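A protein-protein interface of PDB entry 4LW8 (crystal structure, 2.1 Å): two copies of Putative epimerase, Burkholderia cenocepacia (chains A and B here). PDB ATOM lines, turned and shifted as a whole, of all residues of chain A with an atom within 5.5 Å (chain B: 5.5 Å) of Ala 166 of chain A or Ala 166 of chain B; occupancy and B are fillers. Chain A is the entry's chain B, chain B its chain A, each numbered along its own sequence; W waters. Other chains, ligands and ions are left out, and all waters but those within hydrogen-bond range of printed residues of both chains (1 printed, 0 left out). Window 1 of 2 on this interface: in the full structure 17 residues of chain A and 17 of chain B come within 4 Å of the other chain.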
ATOM      1  N   ILE A 111      -7.904 -23.513 -13.913  1.00  0.00           N
ATOM      2  CA  ILE A 111      -7.055 -22.448 -13.377  1.00  0.00           C
ATOM      3  C   ILE A 111      -7.663 -21.771 -12.150  1.00  0.00           C
ATOM      4  O   ILE A 111      -7.069 -21.791 -11.067  1.00  0.00           O
ATOM      5  CB  ILE A 111      -6.762 -21.374 -14.421  1.00  0.00           C
ATOM      6  CG1 ILE A 111      -6.073 -21.987 -15.653  1.00  0.00           C
ATOM      7  CG2 ILE A 111      -5.914 -20.279 -13.808  1.00  0.00           C
ATOM      8  CD1 ILE A 111      -5.935 -20.980 -16.821  1.00  0.00           C
ATOM      9  N   ALA A 161      -4.830 -29.475 -22.045  1.00  0.00           N
ATOM     10  CA  ALA A 161      -3.424 -29.543 -21.642  1.00  0.00           C
ATOM     11  C   ALA A 161      -2.866 -28.142 -21.347  1.00  0.00           C
ATOM     12  O   ALA A 161      -2.113 -27.966 -20.398  1.00  0.00           O
ATOM     13  CB  ALA A 161      -2.597 -30.230 -22.734  1.00  0.00           C
ATOM     14  N   VAL A 162      -3.253 -27.138 -22.140  1.00  0.00           N
ATOM     15  CA  VAL A 162      -2.820 -25.770 -21.844  1.00  0.00           C
ATOM     16  C   VAL A 162      -3.323 -25.362 -20.461  1.00  0.00           C
ATOM     17  O   VAL A 162      -2.564 -24.800 -19.675  1.00  0.00           O
ATOM     18  CB  VAL A 162      -3.308 -24.735 -22.895  1.00  0.00           C
ATOM     19  CG1 VAL A 162      -2.950 -23.325 -22.460  1.00  0.00           C
ATOM     20  CG2 VAL A 162      -2.699 -25.015 -24.275  1.00  0.00           C
ATOM     21  N   SER A 163      -4.578 -25.690 -20.141  1.00  0.00           N
ATOM     22  CA  SER A 163      -5.166 -25.293 -18.857  1.00  0.00           C
ATOM     23  C   SER A 163      -4.451 -25.967 -17.676  1.00  0.00           C
ATOM     24  O   SER A 163      -4.327 -25.395 -16.595  1.00  0.00           O
ATOM     25  CB  SER A 163      -6.675 -25.620 -18.822  1.00  0.00           C
ATOM     26  OG  SER A 163      -6.915 -26.987 -18.505  1.00  0.00           O
ATOM     27  N   LYS A 164      -3.989 -27.189 -17.884  1.00  0.00           N
ATOM     28  CA  LYS A 164      -3.230 -27.905 -16.846  1.00  0.00           C
ATOM     29  C   LYS A 164      -1.870 -27.236 -16.628  1.00  0.00           C
ATOM     30  O   LYS A 164      -1.431 -27.070 -15.489  1.00  0.00           O
ATOM     31  CB  LYS A 164      -3.051 -29.386 -17.239  1.00  0.00           C
ATOM     32  CG  LYS A 164      -4.297 -30.243 -17.004  1.00  0.00           C
ATOM     33  CD  LYS A 164      -4.561 -30.313 -15.501  1.00  0.00           C
ATOM     34  CE  LYS A 164      -5.536 -31.390 -15.108  1.00  0.00           C
ATOM     35  NZ  LYS A 164      -5.731 -31.332 -13.618  1.00  0.00           N
ATOM     36  N   LEU A 165      -1.206 -26.847 -17.721  1.00  0.00           N
ATOM     37  CA  LEU A 165       0.071 -26.136 -17.608  1.00  0.00           C
ATOM     38  C   LEU A 165      -0.119 -24.772 -16.935  1.00  0.00           C
ATOM     39  O   LEU A 165       0.654 -24.372 -16.068  1.00  0.00           O
ATOM     40  CB  LEU A 165       0.722 -25.951 -18.976  1.00  0.00           C
ATOM     41  CG  LEU A 165       2.112 -25.305 -18.953  1.00  0.00           C
ATOM     42  CD1 LEU A 165       3.106 -26.151 -18.138  1.00  0.00           C
ATOM     43  CD2 LEU A 165       2.624 -25.098 -20.395  1.00  0.00           C
ATOM     44  N   ALA A 166      -1.167 -24.064 -17.323  1.00  0.00           N
ATOM     45  CA  ALA A 166      -1.437 -22.757 -16.731  1.00  0.00           C
ATOM     46  C   ALA A 166      -1.724 -22.921 -15.237  1.00  0.00           C
ATOM     47  O   ALA A 166      -1.363 -22.061 -14.420  1.00  0.00           O
ATOM     48  CB  ALA A 166      -2.596 -22.086 -17.442  1.00  0.00           C
ATOM     49  N   MET A 167      -2.391 -24.021 -14.893  1.00  0.00           N
ATOM     50  CA  MET A 167      -2.694 -24.336 -13.492  1.00  0.00           C
ATOM     51  C   MET A 167      -1.415 -24.429 -12.678  1.00  0.00           C
ATOM     52  O   MET A 167      -1.350 -23.938 -11.539  1.00  0.00           O
ATOM     53  CB  MET A 167      -3.471 -25.652 -13.363  1.00  0.00           C
ATOM     54  CG  MET A 167      -3.751 -26.048 -11.906  1.00  0.00           C
ATOM     55  SD  MET A 167      -4.095 -27.807 -11.646  1.00  0.00           S
ATOM     56  CE  MET A 167      -2.450 -28.506 -11.852  1.00  0.00           C
ATOM     57  N   GLU A 168      -0.398 -25.074 -13.259  1.00  0.00           N
ATOM     58  CA  GLU A 168       0.881 -25.231 -12.578  1.00  0.00           C
ATOM     59  C   GLU A 168       1.452 -23.859 -12.262  1.00  0.00           C
ATOM     60  O   GLU A 168       1.889 -23.607 -11.145  1.00  0.00           O
ATOM     61  CB  GLU A 168       1.891 -26.026 -13.423  1.00  0.00           C
ATOM     62  CG  GLU A 168       1.466 -27.467 -13.778  1.00  0.00           C
ATOM     63  CD  GLU A 168       2.600 -28.243 -14.485  1.00  0.00           C
ATOM     64  OE1 GLU A 168       3.721 -27.690 -14.575  1.00  0.00           O
ATOM     65  OE2 GLU A 168       2.381 -29.407 -14.900  1.00  0.00           O
ATOM     66  N   TYR A 169       1.453 -22.974 -13.255  1.00  0.00           N
ATOM     67  CA  TYR A 169       2.051 -21.652 -13.074  1.00  0.00           C
ATOM     68  C   TYR A 169       1.258 -20.783 -12.098  1.00  0.00           C
ATOM     69  O   TYR A 169       1.837 -20.026 -11.312  1.00  0.00           O
ATOM     70  CB  TYR A 169       2.178 -20.931 -14.415  1.00  0.00           C
ATOM     71  CG  TYR A 169       3.357 -21.380 -15.247  1.00  0.00           C
ATOM     72  CD1 TYR A 169       4.661 -21.030 -14.889  1.00  0.00           C
ATOM     73  CD2 TYR A 169       3.170 -22.153 -16.398  1.00  0.00           C
ATOM     74  CE1 TYR A 169       5.738 -21.433 -15.653  1.00  0.00           C
ATOM     75  CE2 TYR A 169       4.257 -22.585 -17.162  1.00  0.00           C
ATOM     76  CZ  TYR A 169       5.522 -22.215 -16.793  1.00  0.00           C
ATOM     77  OH  TYR A 169       6.580 -22.602 -17.560  1.00  0.00           O
ATOM     78  N   ALA A 170      -0.067 -20.856 -12.184  1.00  0.00           N
ATOM     79  CA  ALA A 170      -0.923 -20.101 -11.272  1.00  0.00           C
ATOM     80  C   ALA A 170      -0.722 -20.605  -9.833  1.00  0.00           C
ATOM     81  O   ALA A 170      -0.749 -19.827  -8.889  1.00  0.00           O
ATOM     82  CB  ALA A 170      -2.390 -20.206 -11.685  1.00  0.00           C
ATOM     83  N   ALA A 171      -0.513 -21.908  -9.671  1.00  0.00           N
ATOM     84  CA  ALA A 171      -0.298 -22.470  -8.338  1.00  0.00           C
ATOM     85  C   ALA A 171       1.021 -22.022  -7.725  1.00  0.00           C
ATOM     86  O   ALA A 171       1.106 -21.766  -6.517  1.00  0.00           O
ATOM     87  CB  ALA A 171      -0.345 -23.978  -8.390  1.00  0.00           C
ATOM     88  N   ILE B 111      -6.977 -15.318 -22.071  1.00  0.00           N
ATOM     89  CA  ILE B 111      -6.900 -16.627 -22.735  1.00  0.00           C
ATOM     90  C   ILE B 111      -8.064 -16.851 -23.699  1.00  0.00           C
ATOM     91  O   ILE B 111      -7.854 -17.106 -24.883  1.00  0.00           O
ATOM     92  CB  ILE B 111      -6.893 -17.807 -21.734  1.00  0.00           C
ATOM     93  CG1 ILE B 111      -5.732 -17.688 -20.752  1.00  0.00           C
ATOM     94  CG2 ILE B 111      -6.823 -19.132 -22.481  1.00  0.00           C
ATOM     95  CD1 ILE B 111      -5.828 -18.689 -19.606  1.00  0.00           C
ATOM     96  N   ALA B 161       0.598 -12.073 -15.405  1.00  0.00           N
ATOM     97  CA  ALA B 161       1.728 -12.626 -16.169  1.00  0.00           C
ATOM     98  C   ALA B 161       1.476 -14.093 -16.563  1.00  0.00           C
ATOM     99  O   ALA B 161       1.834 -14.520 -17.664  1.00  0.00           O
ATOM    100  CB  ALA B 161       3.032 -12.485 -15.369  1.00  0.00           C
ATOM    101  N   VAL B 162       0.863 -14.860 -15.661  1.00  0.00           N
ATOM    102  CA  VAL B 162       0.488 -16.246 -15.948  1.00  0.00           C
ATOM    103  C   VAL B 162      -0.505 -16.301 -17.113  1.00  0.00           C
ATOM    104  O   VAL B 162      -0.381 -17.139 -18.018  1.00  0.00           O
ATOM    105  CB  VAL B 162      -0.130 -16.945 -14.720  1.00  0.00           C
ATOM    106  CG1 VAL B 162      -0.666 -18.348 -15.110  1.00  0.00           C
ATOM    107  CG2 VAL B 162       0.899 -17.053 -13.574  1.00  0.00           C
ATOM    108  N   SER B 163      -1.483 -15.400 -17.101  1.00  0.00           N
ATOM    109  CA  SER B 163      -2.522 -15.401 -18.139  1.00  0.00           C
ATOM    110  C   SER B 163      -1.918 -15.065 -19.499  1.00  0.00           C
ATOM    111  O   SER B 163      -2.364 -15.592 -20.521  1.00  0.00           O
ATOM    112  CB  SER B 163      -3.676 -14.431 -17.785  1.00  0.00           C
ATOM    113  OG  SER B 163      -3.387 -13.066 -18.080  1.00  0.00           O
ATOM    114  N   LYS B 164      -0.896 -14.207 -19.518  1.00  0.00           N
ATOM    115  CA  LYS B 164      -0.207 -13.873 -20.777  1.00  0.00           C
ATOM    116  C   LYS B 164       0.565 -15.073 -21.322  1.00  0.00           C
ATOM    117  O   LYS B 164       0.541 -15.351 -22.526  1.00  0.00           O
ATOM    118  CB  LYS B 164       0.743 -12.685 -20.581  1.00  0.00           C
ATOM    119  CG  LYS B 164       0.045 -11.320 -20.519  1.00  0.00           C
ATOM    120  CD  LYS B 164      -0.610 -11.001 -21.870  1.00  0.00           C
ATOM    121  CE  LYS B 164      -0.948  -9.537 -22.012  1.00  0.00           C
ATOM    122  NZ  LYS B 164      -1.592  -9.291 -23.338  1.00  0.00           N
ATOM    123  N   LEU B 165       1.240 -15.790 -20.433  1.00  0.00           N
ATOM    124  CA  LEU B 165       1.952 -17.000 -20.817  1.00  0.00           C
ATOM    125  C   LEU B 165       0.972 -18.055 -21.327  1.00  0.00           C
ATOM    126  O   LEU B 165       1.218 -18.717 -22.341  1.00  0.00           O
ATOM    127  CB  LEU B 165       2.750 -17.560 -19.632  1.00  0.00           C
ATOM    128  CG  LEU B 165       3.615 -18.771 -19.945  1.00  0.00           C
ATOM    129  CD1 LEU B 165       4.631 -18.379 -21.012  1.00  0.00           C
ATOM    130  CD2 LEU B 165       4.321 -19.329 -18.674  1.00  0.00           C
ATOM    131  N   ALA B 166      -0.146 -18.199 -20.622  1.00  0.00           N
ATOM    132  CA  ALA B 166      -1.165 -19.166 -21.002  1.00  0.00           C
ATOM    133  C   ALA B 166      -1.736 -18.794 -22.366  1.00  0.00           C
ATOM    134  O   ALA B 166      -2.014 -19.665 -23.189  1.00  0.00           O
ATOM    135  CB  ALA B 166      -2.261 -19.229 -19.948  1.00  0.00           C
ATOM    136  N   MET B 167      -1.891 -17.492 -22.610  1.00  0.00           N
ATOM    137  CA  MET B 167      -2.347 -17.017 -23.912  1.00  0.00           C
ATOM    138  C   MET B 167      -1.405 -17.508 -25.011  1.00  0.00           C
ATOM    139  O   MET B 167      -1.855 -17.960 -26.075  1.00  0.00           O
ATOM    140  CB  MET B 167      -2.444 -15.484 -23.938  1.00  0.00           C
ATOM    141  CG  MET B 167      -2.894 -14.923 -25.292  1.00  0.00           C
ATOM    142  SD  MET B 167      -2.426 -13.197 -25.591  1.00  0.00           S
ATOM    143  CE  MET B 167      -0.640 -13.407 -25.663  1.00  0.00           C
ATOM    144  N   GLU B 168      -0.098 -17.432 -24.760  1.00  0.00           N
ATOM    145  CA  GLU B 168       0.863 -17.865 -25.773  1.00  0.00           C
ATOM    146  C   GLU B 168       0.631 -19.333 -26.115  1.00  0.00           C
ATOM    147  O   GLU B 168       0.587 -19.699 -27.304  1.00  0.00           O
ATOM    148  CB  GLU B 168       2.316 -17.664 -25.322  1.00  0.00           C
ATOM    149  CG  GLU B 168       2.746 -16.219 -25.014  1.00  0.00           C
ATOM    150  CD  GLU B 168       4.236 -16.137 -24.654  1.00  0.00           C
ATOM    151  OE1 GLU B 168       4.930 -17.167 -24.760  1.00  0.00           O
ATOM    152  OE2 GLU B 168       4.713 -15.056 -24.241  1.00  0.00           O
ATOM    153  N   TYR B 169       0.483 -20.178 -25.090  1.00  0.00           N
ATOM    154  CA  TYR B 169       0.325 -21.613 -25.339  1.00  0.00           C
ATOM    155  C   TYR B 169      -1.019 -21.883 -26.018  1.00  0.00           C
ATOM    156  O   TYR B 169      -1.093 -22.704 -26.927  1.00  0.00           O
ATOM    157  CB  TYR B 169       0.446 -22.431 -24.047  1.00  0.00           C
ATOM    158  CG  TYR B 169       1.885 -22.649 -23.587  1.00  0.00           C
ATOM    159  CD1 TYR B 169       2.733 -23.516 -24.267  1.00  0.00           C
ATOM    160  CD2 TYR B 169       2.398 -21.953 -22.489  1.00  0.00           C
ATOM    161  CE1 TYR B 169       4.041 -23.721 -23.844  1.00  0.00           C
ATOM    162  CE2 TYR B 169       3.704 -22.125 -22.081  1.00  0.00           C
ATOM    163  CZ  TYR B 169       4.516 -23.011 -22.757  1.00  0.00           C
ATOM    164  OH  TYR B 169       5.800 -23.182 -22.341  1.00  0.00           O
ATOM    165  N   ALA B 170      -2.072 -21.182 -25.589  1.00  0.00           N
ATOM    166  CA  ALA B 170      -3.395 -21.360 -26.198  1.00  0.00           C
ATOM    167  C   ALA B 170      -3.362 -20.953 -27.666  1.00  0.00           C
ATOM    168  O   ALA B 170      -3.967 -21.600 -28.514  1.00  0.00           O
ATOM    169  CB  ALA B 170      -4.460 -20.541 -25.448  1.00  0.00           C
ATOM    170  N   ALA B 171      -2.620 -19.899 -27.963  1.00  0.00           N
ATOM    171  CA  ALA B 171      -2.544 -19.400 -29.335  1.00  0.00           C
ATOM    172  C   ALA B 171      -1.803 -20.354 -30.280  1.00  0.00           C
ATOM    173  O   ALA B 171      -2.153 -20.485 -31.450  1.00  0.00           O
ATOM    174  CB  ALA B 171      -1.893 -18.021 -29.355  1.00  0.00           C
HETATM  175  O   HOH W   1       6.827 -22.808 -20.121  1.00  0.00           O
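Ile 111 of chain B touches its own counterpart, Ile 111 of chain A.
Val 162 of chain A touches Ala 166 of chain B, and with the chains exchanged Ala 166 of chain A touches Val 162 of chain B.
Val 162 of chain A touches Ala 170 of chain B, and with the chains exchanged Ala 170 of chain A touches Val 162 of chain B.
Ala 166 of chain A touches its own counterpart, Ala 166 of chain B.
12 positions are printed for both chains.
Among the printed residues, merely in contact across the chains: Leu 165 of chain A with Tyr 169 of chain B, Tyr 169 of chain A with Leu 165 of chain B, Ile 111 of chain A with Ile 111 of chain B, Ala 166 of chain A with Ala 166 of chain B, Ala 166 of chain A with Val 162 of chain B, Val 162 of chain A with Ala 166 of chain B, Tyr 169 of chain A with Val 162 of chain B, Val 162 of chain A with Tyr 169 of chain B, Val 162 of chain A with Ala 170 of chain B and Ala 170 of chain A with Val 162 of chain B.
Printed residues of chain B that touch a printed residue of chain A: Ile 111, Val 162, Leu 165, Ala 166, Tyr 169 and Ala 170.
Hydrophobic or aromatic side chains of chain B that line the printed part of chain A: Ile 111, Val 162, Leu 165, Ala 166 and Tyr 169.
Ala 166 of chain A touches two residues of chain B.
Ala 166 of chain B touches two residues of chain A.
Printed residues of chain A within 4 Å of Ile 111 of chain B: Ile 111 (3.6 Å).
Of the printed residues of chain B, Leu 165 of chain A touches Tyr 169.
Of the printed residues of chain A, Val 162 of chain B touches Ala 166, Tyr 169 and Ala 170.
Printed residues of chain A within 4 Å of Tyr 169 of chain B: Val 162 (3.9 Å) and Leu 165 (3.6 Å).
Of the printed residues of chain B, Tyr 169 of chain A touches Val 162 (3.9 Å) and Leu 165 (3.6 Å).
The nearest printed residue of chain A that does not touch Tyr 169 of chain B is Tyr 169 of chain A (4.9 Å).
Water W1 lies within hydrogen-bond range of OH of Tyr 169 of chain B (2.5 Å) and OH of Tyr 169 of chain A (2.6 Å).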
